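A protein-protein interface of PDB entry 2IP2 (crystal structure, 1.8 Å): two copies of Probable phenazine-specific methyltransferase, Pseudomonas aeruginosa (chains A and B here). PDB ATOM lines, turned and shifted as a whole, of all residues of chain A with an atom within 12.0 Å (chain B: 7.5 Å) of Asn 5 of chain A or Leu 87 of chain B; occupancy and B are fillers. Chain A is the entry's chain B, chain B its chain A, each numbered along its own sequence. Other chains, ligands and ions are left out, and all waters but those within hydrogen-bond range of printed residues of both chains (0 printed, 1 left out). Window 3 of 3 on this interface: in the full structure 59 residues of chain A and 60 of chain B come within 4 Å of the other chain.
Of the printed residues of chain B, Asn 5 of chain A touches Leu 87 (3.998 Å).
Of the printed residues of chain B, Ala 8 of chain A touches Pro 83 (3.7 Å), Thr 84 (3.9 Å) and Leu 87 (3.9 Å).
Asn 11 of chain A touches none of the printed residues of chain B.
Of the printed residues of chain B, Ile 13 of chain A touches Phe 95 and Met 98.
Gln 14 of chain A touches none of the printed residues of chain B.
Pro 83 of chain B touches just one residue of chain A: Ala 8.
Printed residues of chain A within 4 Å of Thr 84 of chain B: Ala 8 (3.9 Å) and Leu 12 (3.8 Å).
Ser 85 of chain B touches none of the printed residues of chain A.
No residue of chain A comes within 4 Å of His 86 of chain B.
Of the printed residues of chain A, Leu 87 of chain B touches Asn 5 (3.998 Å), Ala 8 (3.9 Å), Ala 9 (3.7 Å) and Leu 12 (3.8 Å).
Leu 88 of chain B touches one residue of chain A.
Of chain A, only Ala 9 (3.7 Å), Leu 12 (3.7 Å) and Ile 13 (3.5 Å) come within 4 Å of Phe 95 of chain B.
Of the printed residues of chain A, Met 98 of chain B touches Ile 13.
Printed residues of chain A within 4 Å of Val 99 of chain B: Val 16.
Printed residues of chain A within 4 Å of Leu 155 of chain B: Ala 9.
The nearest printed residue of chain B that does not touch Val 16 of chain A is Met 98 of chain B (4.3 Å).
Hydrophobic or aromatic side chains of chain B within 4 Å of the printed part of chain A: Pro 83, Leu 87, Leu 88, Phe 95, Met 98, Val 99 and Leu 155.
Of the 12 printed residues of chain A, 6 touch a printed residue of chain B.
Printed residues of chain A that touch a printed residue of chain B: Asn 5, Ala 8, Ala 9, Leu 12, Ile 13 and Val 16.
Hydrophobic or aromatic side chains of chain A within 4 Å of the printed part of chain B: Ala 8, Ala 9, Leu 12, Ile 13 and Val 16.
OD1 of Asn 5 of chain A touches CD2 of Leu 87 of chain B, 3.998 Å away.
Pro 83 of chain B touches Ala 8 of chain A.
O of Ala 8 of chain A touches OG1 of Thr 84 of chain B, 3.9 Å away.
Leu 87 of chain B touches Ala 8 of chain A (CD1 to O, 3.9 Å).
Phe 95 of chain B touches Ala 9 of chain A (CZ to CB, 3.7 Å).
Leu 12 of chain A touches Thr 84 of chain B (CB to CG2, 3.8 Å).
CD2 of Leu 88 of chain B touches CD2 of Leu 12 of chain A, 3.97 Å away.
CG1 of Ile 13 of chain A touches CE2 of Phe 95 of chain B, 3.5 Å away.
CD1 of Ile 13 of chain A touches CE of Met 98 of chain B, at 3.4 Å.
CG2 of Val 99 of chain B touches CG2 of Val 16 of chain A (3.9 Å).
No position is printed for both chains.
Of the 14 pairs that touch across the chains among the printed residues, none has its exchanged pair printed and touching as well.
The backbone NH (N) of Phe 95 of chain B lies within hydrogen-bond range of the backbone carbonyl oxygen (O) of Leu 87 of chain B.
O of Leu 87 of chain B sits at hydrogen-bond distance from N of Arg 96 of chain B (3.4 Å).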
ATOM      1  N   ASN A   5       6.057  -8.187  13.356  1.00  0.00           N
ATOM      2  CA  ASN A   5       7.232  -7.623  14.085  1.00  0.00           C
ATOM      3  C   ASN A   5       7.277  -6.076  14.089  1.00  0.00           C
ATOM      4  O   ASN A   5       7.662  -5.492  15.098  1.00  0.00           O
ATOM      5  CB  ASN A   5       8.563  -8.210  13.583  1.00  0.00           C
ATOM      6  CG  ASN A   5       9.608  -8.350  14.712  1.00  0.00           C
ATOM      7  OD1 ASN A   5       9.262  -8.734  15.830  1.00  0.00           O
ATOM      8  ND2 ASN A   5      10.892  -8.053  14.411  1.00  0.00           N
ATOM      9  N   LEU A   6       6.875  -5.439  12.978  1.00  0.00           N
ATOM     10  CA  LEU A   6       6.778  -3.954  12.854  1.00  0.00           C
ATOM     11  C   LEU A   6       5.692  -3.309  13.714  1.00  0.00           C
ATOM     12  O   LEU A   6       5.957  -2.367  14.469  1.00  0.00           O
ATOM     13  CB  LEU A   6       6.418  -3.543  11.423  1.00  0.00           C
ATOM     14  CG  LEU A   6       7.336  -3.805  10.246  1.00  0.00           C
ATOM     15  CD1 LEU A   6       6.448  -4.220   9.049  1.00  0.00           C
ATOM     16  CD2 LEU A   6       8.156  -2.569   9.964  1.00  0.00           C
ATOM     17  N   ALA A   7       4.455  -3.755  13.511  1.00  0.00           N
ATOM     18  CA  ALA A   7       3.344  -3.318  14.344  1.00  0.00           C
ATOM     19  C   ALA A   7       3.660  -3.600  15.821  1.00  0.00           C
ATOM     20  O   ALA A   7       3.366  -2.757  16.679  1.00  0.00           O
ATOM     21  CB  ALA A   7       2.052  -4.025  13.932  1.00  0.00           C
ATOM     22  N   ALA A   8       4.258  -4.774  16.086  1.00  0.00           N
ATOM     23  CA  ALA A   8       4.645  -5.224  17.435  1.00  0.00           C
ATOM     24  C   ALA A   8       5.748  -4.352  18.072  1.00  0.00           C
ATOM     25  O   ALA A   8       5.664  -4.044  19.252  1.00  0.00           O
ATOM     26  CB  ALA A   8       5.051  -6.693  17.429  1.00  0.00           C
ATOM     27  N   ALA A   9       6.769  -3.980  17.295  1.00  0.00           N
ATOM     28  CA  ALA A   9       7.782  -3.061  17.769  1.00  0.00           C
ATOM     29  C   ALA A   9       7.133  -1.700  18.000  1.00  0.00           C
ATOM     30  O   ALA A   9       7.420  -1.050  19.001  1.00  0.00           O
ATOM     31  CB  ALA A   9       8.927  -2.945  16.768  1.00  0.00           C
ATOM     32  N   ARG A  10       6.242  -1.277  17.104  1.00  0.00           N
ATOM     33  CA  ARG A  10       5.644   0.043  17.291  1.00  0.00           C
ATOM     34  C   ARG A  10       4.743   0.052  18.529  1.00  0.00           C
ATOM     35  O   ARG A  10       4.762   1.003  19.302  1.00  0.00           O
ATOM     36  CB  ARG A  10       4.941   0.505  16.028  1.00  0.00           C
ATOM     37  CG  ARG A  10       3.857   1.536  16.197  1.00  0.00           C
ATOM     38  CD  ARG A  10       3.256   1.817  14.818  1.00  0.00           C
ATOM     39  NE  ARG A  10       4.256   1.662  13.746  1.00  0.00           N
ATOM     40  CZ  ARG A  10       4.212   0.721  12.801  1.00  0.00           C
ATOM     41  NH1 ARG A  10       3.214  -0.163  12.762  1.00  0.00           N
ATOM     42  NH2 ARG A  10       5.166   0.673  11.876  1.00  0.00           N
ATOM     43  N   ASN A  11       3.980  -1.015  18.742  1.00  0.00           N
ATOM     44  CA  ASN A  11       3.137  -0.997  19.933  1.00  0.00           C
ATOM     45  C   ASN A  11       3.958  -1.067  21.206  1.00  0.00           C
ATOM     46  O   ASN A  11       3.659  -0.373  22.153  1.00  0.00           O
ATOM     47  CB  ASN A  11       2.032  -2.038  19.936  1.00  0.00           C
ATOM     48  CG  ASN A  11       1.147  -1.886  21.150  1.00  0.00           C
ATOM     49  OD1 ASN A  11       0.458  -0.861  21.318  1.00  0.00           O
ATOM     50  ND2 ASN A  11       1.212  -2.857  22.030  1.00  0.00           N
ATOM     51  N   LEU A  12       5.018  -1.867  21.194  1.00  0.00           N
ATOM     52  CA  LEU A  12       5.870  -1.999  22.335  1.00  0.00           C
ATOM     53  C   LEU A  12       6.537  -0.678  22.684  1.00  0.00           C
ATOM     54  O   LEU A  12       6.702  -0.340  23.855  1.00  0.00           O
ATOM     55  CB  LEU A  12       6.938  -3.070  22.125  1.00  0.00           C
ATOM     56  CG  LEU A  12       7.877  -3.224  23.324  1.00  0.00           C
ATOM     57  CD1 LEU A  12       7.044  -3.591  24.625  1.00  0.00           C
ATOM     58  CD2 LEU A  12       8.939  -4.215  23.037  1.00  0.00           C
ATOM     59  N   ILE A  13       6.962   0.058  21.676  1.00  0.00           N
ATOM     60  CA  ILE A  13       7.658   1.278  21.957  1.00  0.00           C
ATOM     61  C   ILE A  13       6.683   2.292  22.555  1.00  0.00           C
ATOM     62  O   ILE A  13       7.076   3.070  23.435  1.00  0.00           O
ATOM     63  CB  ILE A  13       8.364   1.822  20.688  1.00  0.00           C
ATOM     64  CG1 ILE A  13       9.580   0.973  20.375  1.00  0.00           C
ATOM     65  CG2 ILE A  13       8.727   3.297  20.871  1.00  0.00           C
ATOM     66  CD1 ILE A  13      10.813   1.337  21.216  1.00  0.00           C
ATOM     67  N   GLN A  14       5.450   2.301  22.059  1.00  0.00           N
ATOM     68  CA  GLN A  14       4.396   3.162  22.618  1.00  0.00           C
ATOM     69  C   GLN A  14       4.286   2.908  24.127  1.00  0.00           C
ATOM     70  O   GLN A  14       4.169   3.832  24.916  1.00  0.00           O
ATOM     71  CB  GLN A  14       3.048   2.833  21.970  1.00  0.00           C
ATOM     72  CG  GLN A  14       1.923   3.876  22.244  1.00  0.00           C
ATOM     73  CD  GLN A  14       1.328   3.793  23.680  1.00  0.00           C
ATOM     74  OE1 GLN A  14       1.077   2.717  24.205  1.00  0.00           O
ATOM     75  NE2 GLN A  14       1.084   4.937  24.271  1.00  0.00           N
ATOM     76  N   VAL A  15       4.268   1.632  24.494  1.00  0.00           N
ATOM     77  CA  VAL A  15       4.019   1.273  25.906  1.00  0.00           C
ATOM     78  C   VAL A  15       5.245   1.671  26.734  1.00  0.00           C
ATOM     79  O   VAL A  15       5.099   2.235  27.801  1.00  0.00           O
ATOM     80  CB  VAL A  15       3.720  -0.260  26.071  1.00  0.00           C
ATOM     81  CG1 VAL A  15       3.628  -0.619  27.569  1.00  0.00           C
ATOM     82  CG2 VAL A  15       2.416  -0.562  25.441  1.00  0.00           C
ATOM     83  N   VAL A  16       6.446   1.303  26.253  1.00  0.00           N
ATOM     84  CA  VAL A  16       7.727   1.640  26.928  1.00  0.00           C
ATOM     85  C   VAL A  16       7.882   3.156  27.178  1.00  0.00           C
ATOM     86  O   VAL A  16       8.248   3.582  28.294  1.00  0.00           O
ATOM     87  CB  VAL A  16       8.931   1.063  26.127  1.00  0.00           C
ATOM     88  CG1 VAL A  16      10.321   1.600  26.700  1.00  0.00           C
ATOM     89  CG2 VAL A  16       8.867  -0.547  26.117  1.00  0.00           C
ATOM     90  N   THR B  29      10.427  -7.509  32.140  1.00  0.00           N
ATOM     91  CA  THR B  29      11.762  -7.594  31.514  1.00  0.00           C
ATOM     92  C   THR B  29      12.876  -7.911  32.532  1.00  0.00           C
ATOM     93  O   THR B  29      13.629  -8.870  32.333  1.00  0.00           O
ATOM     94  CB  THR B  29      12.063  -6.349  30.616  1.00  0.00           C
ATOM     95  OG1 THR B  29      10.993  -6.234  29.687  1.00  0.00           O
ATOM     96  CG2 THR B  29      13.441  -6.553  29.804  1.00  0.00           C
ATOM     97  N   ALA B  34       9.485 -13.336  29.907  1.00  0.00           N
ATOM     98  CA  ALA B  34       9.403 -13.811  28.554  1.00  0.00           C
ATOM     99  C   ALA B  34      10.316 -15.017  28.269  1.00  0.00           C
ATOM    100  O   ALA B  34       9.898 -15.928  27.544  1.00  0.00           O
ATOM    101  CB  ALA B  34       9.730 -12.669  27.591  1.00  0.00           C
ATOM    102  N   ASN B  81       4.307 -16.458  24.824  1.00  0.00           N
ATOM    103  CA  ASN B  81       4.715 -15.193  24.212  1.00  0.00           C
ATOM    104  C   ASN B  81       3.816 -14.743  23.046  1.00  0.00           C
ATOM    105  O   ASN B  81       3.102 -15.568  22.442  1.00  0.00           O
ATOM    106  CB  ASN B  81       6.199 -15.294  23.812  1.00  0.00           C
ATOM    107  CG  ASN B  81       7.108 -15.121  25.016  1.00  0.00           C
ATOM    108  OD1 ASN B  81       6.992 -14.119  25.740  1.00  0.00           O
ATOM    109  ND2 ASN B  81       7.965 -16.117  25.286  1.00  0.00           N
ATOM    110  N   THR B  82       3.868 -13.434  22.754  1.00  0.00           N
ATOM    111  CA  THR B  82       3.207 -12.795  21.616  1.00  0.00           C
ATOM    112  C   THR B  82       4.320 -12.136  20.773  1.00  0.00           C
ATOM    113  O   THR B  82       5.473 -12.058  21.240  1.00  0.00           O
ATOM    114  CB  THR B  82       2.190 -11.745  22.096  1.00  0.00           C
ATOM    115  OG1 THR B  82       2.849 -10.753  22.914  1.00  0.00           O
ATOM    116  CG2 THR B  82       1.005 -12.414  22.886  1.00  0.00           C
ATOM    117  N   PRO B  83       4.030 -11.711  19.516  1.00  0.00           N
ATOM    118  CA  PRO B  83       5.074 -10.919  18.842  1.00  0.00           C
ATOM    119  C   PRO B  83       5.663  -9.758  19.696  1.00  0.00           C
ATOM    120  O   PRO B  83       6.873  -9.514  19.623  1.00  0.00           O
ATOM    121  CB  PRO B  83       4.387 -10.357  17.580  1.00  0.00           C
ATOM    122  CG  PRO B  83       3.073 -11.125  17.443  1.00  0.00           C
ATOM    123  CD  PRO B  83       2.856 -11.986  18.656  1.00  0.00           C
ATOM    124  N   THR B  84       4.831  -9.100  20.497  1.00  0.00           N
ATOM    125  CA  THR B  84       5.292  -8.010  21.361  1.00  0.00           C
ATOM    126  C   THR B  84       6.260  -8.553  22.457  1.00  0.00           C
ATOM    127  O   THR B  84       7.363  -8.016  22.621  1.00  0.00           O
ATOM    128  CB  THR B  84       4.113  -7.200  22.012  1.00  0.00           C
ATOM    129  OG1 THR B  84       3.313  -6.600  20.982  1.00  0.00           O
ATOM    130  CG2 THR B  84       4.670  -6.053  22.840  1.00  0.00           C
ATOM    131  N   SER B  85       5.858  -9.608  23.176  1.00  0.00           N
ATOM    132  CA  SER B  85       6.703 -10.112  24.289  1.00  0.00           C
ATOM    133  C   SER B  85       8.004 -10.816  23.837  1.00  0.00           C
ATOM    134  O   SER B  85       9.011 -10.823  24.536  1.00  0.00           O
ATOM    135  CB  SER B  85       5.908 -10.957  25.279  1.00  0.00           C
ATOM    136  OG  SER B  85       5.556 -12.242  24.767  1.00  0.00           O
ATOM    137  N   HIS B  86       7.970 -11.424  22.661  1.00  0.00           N
ATOM    138  CA  HIS B  86       9.210 -11.927  22.013  1.00  0.00           C
ATOM    139  C   HIS B  86      10.285 -10.858  21.920  1.00  0.00           C
ATOM    140  O   HIS B  86      11.463 -11.128  22.050  1.00  0.00           O
ATOM    141  CB  HIS B  86       8.877 -12.509  20.628  1.00  0.00           C
ATOM    142  CG  HIS B  86       8.333 -13.903  20.676  1.00  0.00           C
ATOM    143  ND1 HIS B  86       8.982 -14.933  21.322  1.00  0.00           N
ATOM    144  CD2 HIS B  86       7.223 -14.447  20.120  1.00  0.00           C
ATOM    145  CE1 HIS B  86       8.290 -16.047  21.173  1.00  0.00           C
ATOM    146  NE2 HIS B  86       7.224 -15.779  20.444  1.00  0.00           N
ATOM    147  N   LEU B  87       9.861  -9.615  21.753  1.00  0.00           N
ATOM    148  CA  LEU B  87      10.827  -8.513  21.730  1.00  0.00           C
ATOM    149  C   LEU B  87      11.459  -8.217  23.078  1.00  0.00           C
ATOM    150  O   LEU B  87      12.440  -7.457  23.169  1.00  0.00           O
ATOM    151  CB  LEU B  87      10.160  -7.254  21.183  1.00  0.00           C
ATOM    152  CG  LEU B  87       9.830  -7.255  19.685  1.00  0.00           C
ATOM    153  CD1 LEU B  87       8.919  -6.110  19.457  1.00  0.00           C
ATOM    154  CD2 LEU B  87      11.123  -7.025  18.928  1.00  0.00           C
ATOM    155  N   LEU B  88      10.908  -8.799  24.137  1.00  0.00           N
ATOM    156  CA  LEU B  88      11.513  -8.643  25.444  1.00  0.00           C
ATOM    157  C   LEU B  88      12.508  -9.723  25.803  1.00  0.00           C
ATOM    158  O   LEU B  88      13.197  -9.628  26.845  1.00  0.00           O
ATOM    159  CB  LEU B  88      10.426  -8.566  26.546  1.00  0.00           C
ATOM    160  CG  LEU B  88       9.313  -7.541  26.373  1.00  0.00           C
ATOM    161  CD1 LEU B  88       8.284  -7.803  27.438  1.00  0.00           C
ATOM    162  CD2 LEU B  88       9.852  -6.088  26.417  1.00  0.00           C
ATOM    163  N   ARG B  89      12.552 -10.800  24.996  1.00  0.00           N
ATOM    164  CA  ARG B  89      13.420 -11.945  25.306  1.00  0.00           C
ATOM    165  C   ARG B  89      14.898 -11.624  25.174  1.00  0.00           C
ATOM    166  O   ARG B  89      15.311 -10.725  24.426  1.00  0.00           O
ATOM    167  CB  ARG B  89      13.090 -13.147  24.387  1.00  0.00           C
ATOM    168  CG  ARG B  89      11.759 -13.869  24.686  1.00  0.00           C
ATOM    169  CD  ARG B  89      11.312 -14.717  23.430  1.00  0.00           C
ATOM    170  NE  ARG B  89      12.127 -15.887  23.285  1.00  0.00           N
ATOM    171  CZ  ARG B  89      12.530 -16.415  22.145  1.00  0.00           C
ATOM    172  NH1 ARG B  89      12.190 -15.890  20.961  1.00  0.00           N
ATOM    173  NH2 ARG B  89      13.284 -17.496  22.211  1.00  0.00           N
ATOM    174  N   ASP B  90      15.702 -12.392  25.869  1.00  0.00           N
ATOM    175  CA  ASP B  90      17.128 -12.190  25.866  1.00  0.00           C
ATOM    176  C   ASP B  90      17.725 -12.849  24.603  1.00  0.00           C
ATOM    177  O   ASP B  90      18.341 -13.886  24.690  1.00  0.00           O
ATOM    178  CB  ASP B  90      17.695 -12.784  27.158  1.00  0.00           C
ATOM    179  CG  ASP B  90      19.166 -12.474  27.351  1.00  0.00           C
ATOM    180  OD1 ASP B  90      19.716 -11.627  26.602  1.00  0.00           O
ATOM    181  OD2 ASP B  90      19.765 -13.116  28.242  1.00  0.00           O
ATOM    182  N   VAL B  91      17.491 -12.222  23.444  1.00  0.00           N
ATOM    183  CA  VAL B  91      17.924 -12.717  22.141  1.00  0.00           C
ATOM    184  C   VAL B  91      18.550 -11.537  21.357  1.00  0.00           C
ATOM    185  O   VAL B  91      18.178 -10.370  21.538  1.00  0.00           O
ATOM    186  CB  VAL B  91      16.746 -13.406  21.356  1.00  0.00           C
ATOM    187  CG1 VAL B  91      16.373 -14.752  22.023  1.00  0.00           C
ATOM    188  CG2 VAL B  91      15.530 -12.482  21.278  1.00  0.00           C
ATOM    189  N   GLY B  93      18.628  -9.508  18.707  1.00  0.00           N
ATOM    190  CA  GLY B  93      18.072  -8.234  18.257  1.00  0.00           C
ATOM    191  C   GLY B  93      16.780  -7.795  18.927  1.00  0.00           C
ATOM    192  O   GLY B  93      15.900  -7.243  18.269  1.00  0.00           O
ATOM    193  N   SER B  94      16.640  -8.060  20.235  1.00  0.00           N
ATOM    194  CA  SER B  94      15.372  -7.737  20.908  1.00  0.00           C
ATOM    195  C   SER B  94      15.430  -6.307  21.451  1.00  0.00           C
ATOM    196  O   SER B  94      16.471  -5.639  21.398  1.00  0.00           O
ATOM    197  CB  SER B  94      15.147  -8.696  22.064  1.00  0.00           C
ATOM    198  OG  SER B  94      16.186  -8.505  23.014  1.00  0.00           O
ATOM    199  N   PHE B  95      14.310  -5.869  22.026  1.00  0.00           N
ATOM    200  CA  PHE B  95      14.238  -4.572  22.742  1.00  0.00           C
ATOM    201  C   PHE B  95      14.618  -4.684  24.221  1.00  0.00           C
ATOM    202  O   PHE B  95      14.567  -3.686  24.979  1.00  0.00           O
ATOM    203  CB  PHE B  95      12.837  -4.017  22.594  1.00  0.00           C
ATOM    204  CG  PHE B  95      12.549  -3.473  21.224  1.00  0.00           C
ATOM    205  CD1 PHE B  95      13.300  -3.864  20.130  1.00  0.00           C
ATOM    206  CD2 PHE B  95      11.532  -2.543  21.027  1.00  0.00           C
ATOM    207  CE1 PHE B  95      13.030  -3.359  18.852  1.00  0.00           C
ATOM    208  CE2 PHE B  95      11.262  -2.010  19.736  1.00  0.00           C
ATOM    209  CZ  PHE B  95      12.007  -2.428  18.658  1.00  0.00           C
ATOM    210  N   ARG B  96      15.047  -5.895  24.609  1.00  0.00           N
ATOM    211  CA  ARG B  96      15.253  -6.192  26.039  1.00  0.00           C
ATOM    212  C   ARG B  96      16.194  -5.193  26.702  1.00  0.00           C
ATOM    213  O   ARG B  96      15.847  -4.591  27.707  1.00  0.00           O
ATOM    214  CB  ARG B  96      15.766  -7.631  26.264  1.00  0.00           C
ATOM    215  CG  ARG B  96      16.235  -7.860  27.678  1.00  0.00           C
ATOM    216  CD  ARG B  96      16.700  -9.338  28.010  1.00  0.00           C
ATOM    217  NE  ARG B  96      17.623  -9.276  29.153  1.00  0.00           N
ATOM    218  CZ  ARG B  96      17.272  -9.385  30.430  1.00  0.00           C
ATOM    219  NH1 ARG B  96      16.015  -9.622  30.771  1.00  0.00           N
ATOM    220  NH2 ARG B  96      18.202  -9.287  31.363  1.00  0.00           N
ATOM    221  N   ASP B  97      17.409  -5.023  26.165  1.00  0.00           N
ATOM    222  CA  ASP B  97      18.358  -4.104  26.800  1.00  0.00           C
ATOM    223  C   ASP B  97      17.910  -2.662  26.727  1.00  0.00           C
ATOM    224  O   ASP B  97      18.301  -1.880  27.571  1.00  0.00           O
ATOM    225  CB  ASP B  97      19.721  -4.219  26.118  1.00  0.00           C
ATOM    226  CG  ASP B  97      20.327  -5.571  26.401  1.00  0.00           C
ATOM    227  OD1 ASP B  97      20.369  -5.935  27.612  1.00  0.00           O
ATOM    228  OD2 ASP B  97      20.641  -6.279  25.443  1.00  0.00           O
ATOM    229  N   MET B  98      17.192  -2.309  25.670  1.00  0.00           N
ATOM    230  CA  MET B  98      16.630  -0.933  25.574  1.00  0.00           C
ATOM    231  C   MET B  98      15.593  -0.700  26.697  1.00  0.00           C
ATOM    232  O   MET B  98      15.658   0.307  27.434  1.00  0.00           O
ATOM    233  CB  MET B  98      16.003  -0.683  24.194  1.00  0.00           C
ATOM    234  CG  MET B  98      15.535   0.759  23.985  1.00  0.00           C
ATOM    235  SD  MET B  98      14.303   0.922  22.704  1.00  0.00           S
ATOM    236  CE  MET B  98      12.950   0.131  23.604  1.00  0.00           C
ATOM    237  N   VAL B  99      14.687  -1.652  26.881  1.00  0.00           N
ATOM    238  CA  VAL B  99      13.676  -1.552  27.982  1.00  0.00           C
ATOM    239  C   VAL B  99      14.338  -1.331  29.355  1.00  0.00           C
ATOM    240  O   VAL B  99      13.911  -0.490  30.167  1.00  0.00           O
ATOM    241  CB  VAL B  99      12.751  -2.811  28.017  1.00  0.00           C
ATOM    242  CG1 VAL B  99      11.874  -2.858  29.312  1.00  0.00           C
ATOM    243  CG2 VAL B  99      11.871  -2.900  26.708  1.00  0.00           C
ATOM    244  N   ALA B 152      18.443  -1.827  19.628  1.00  0.00           N
ATOM    245  CA  ALA B 152      17.023  -1.911  19.252  1.00  0.00           C
ATOM    246  C   ALA B 152      16.786  -1.200  17.907  1.00  0.00           C
ATOM    247  O   ALA B 152      15.919  -1.595  17.113  1.00  0.00           O
ATOM    248  CB  ALA B 152      16.124  -1.329  20.359  1.00  0.00           C
ATOM    249  N   LEU B 155      16.915  -2.333  13.933  1.00  0.00           N
ATOM    250  CA  LEU B 155      15.707  -2.508  13.123  1.00  0.00           C
ATOM    251  C   LEU B 155      15.771  -1.620  11.874  1.00  0.00           C
ATOM    252  O   LEU B 155      15.446  -2.066  10.767  1.00  0.00           O
ATOM    253  CB  LEU B 155      14.430  -2.215  13.932  1.00  0.00           C
ATOM    254  CG  LEU B 155      13.645  -3.389  14.531  1.00  0.00           C
ATOM    255  CD1 LEU B 155      14.348  -4.031  15.724  1.00  0.00           C
ATOM    256  CD2 LEU B 155      12.226  -2.977  14.919  1.00  0.00           C
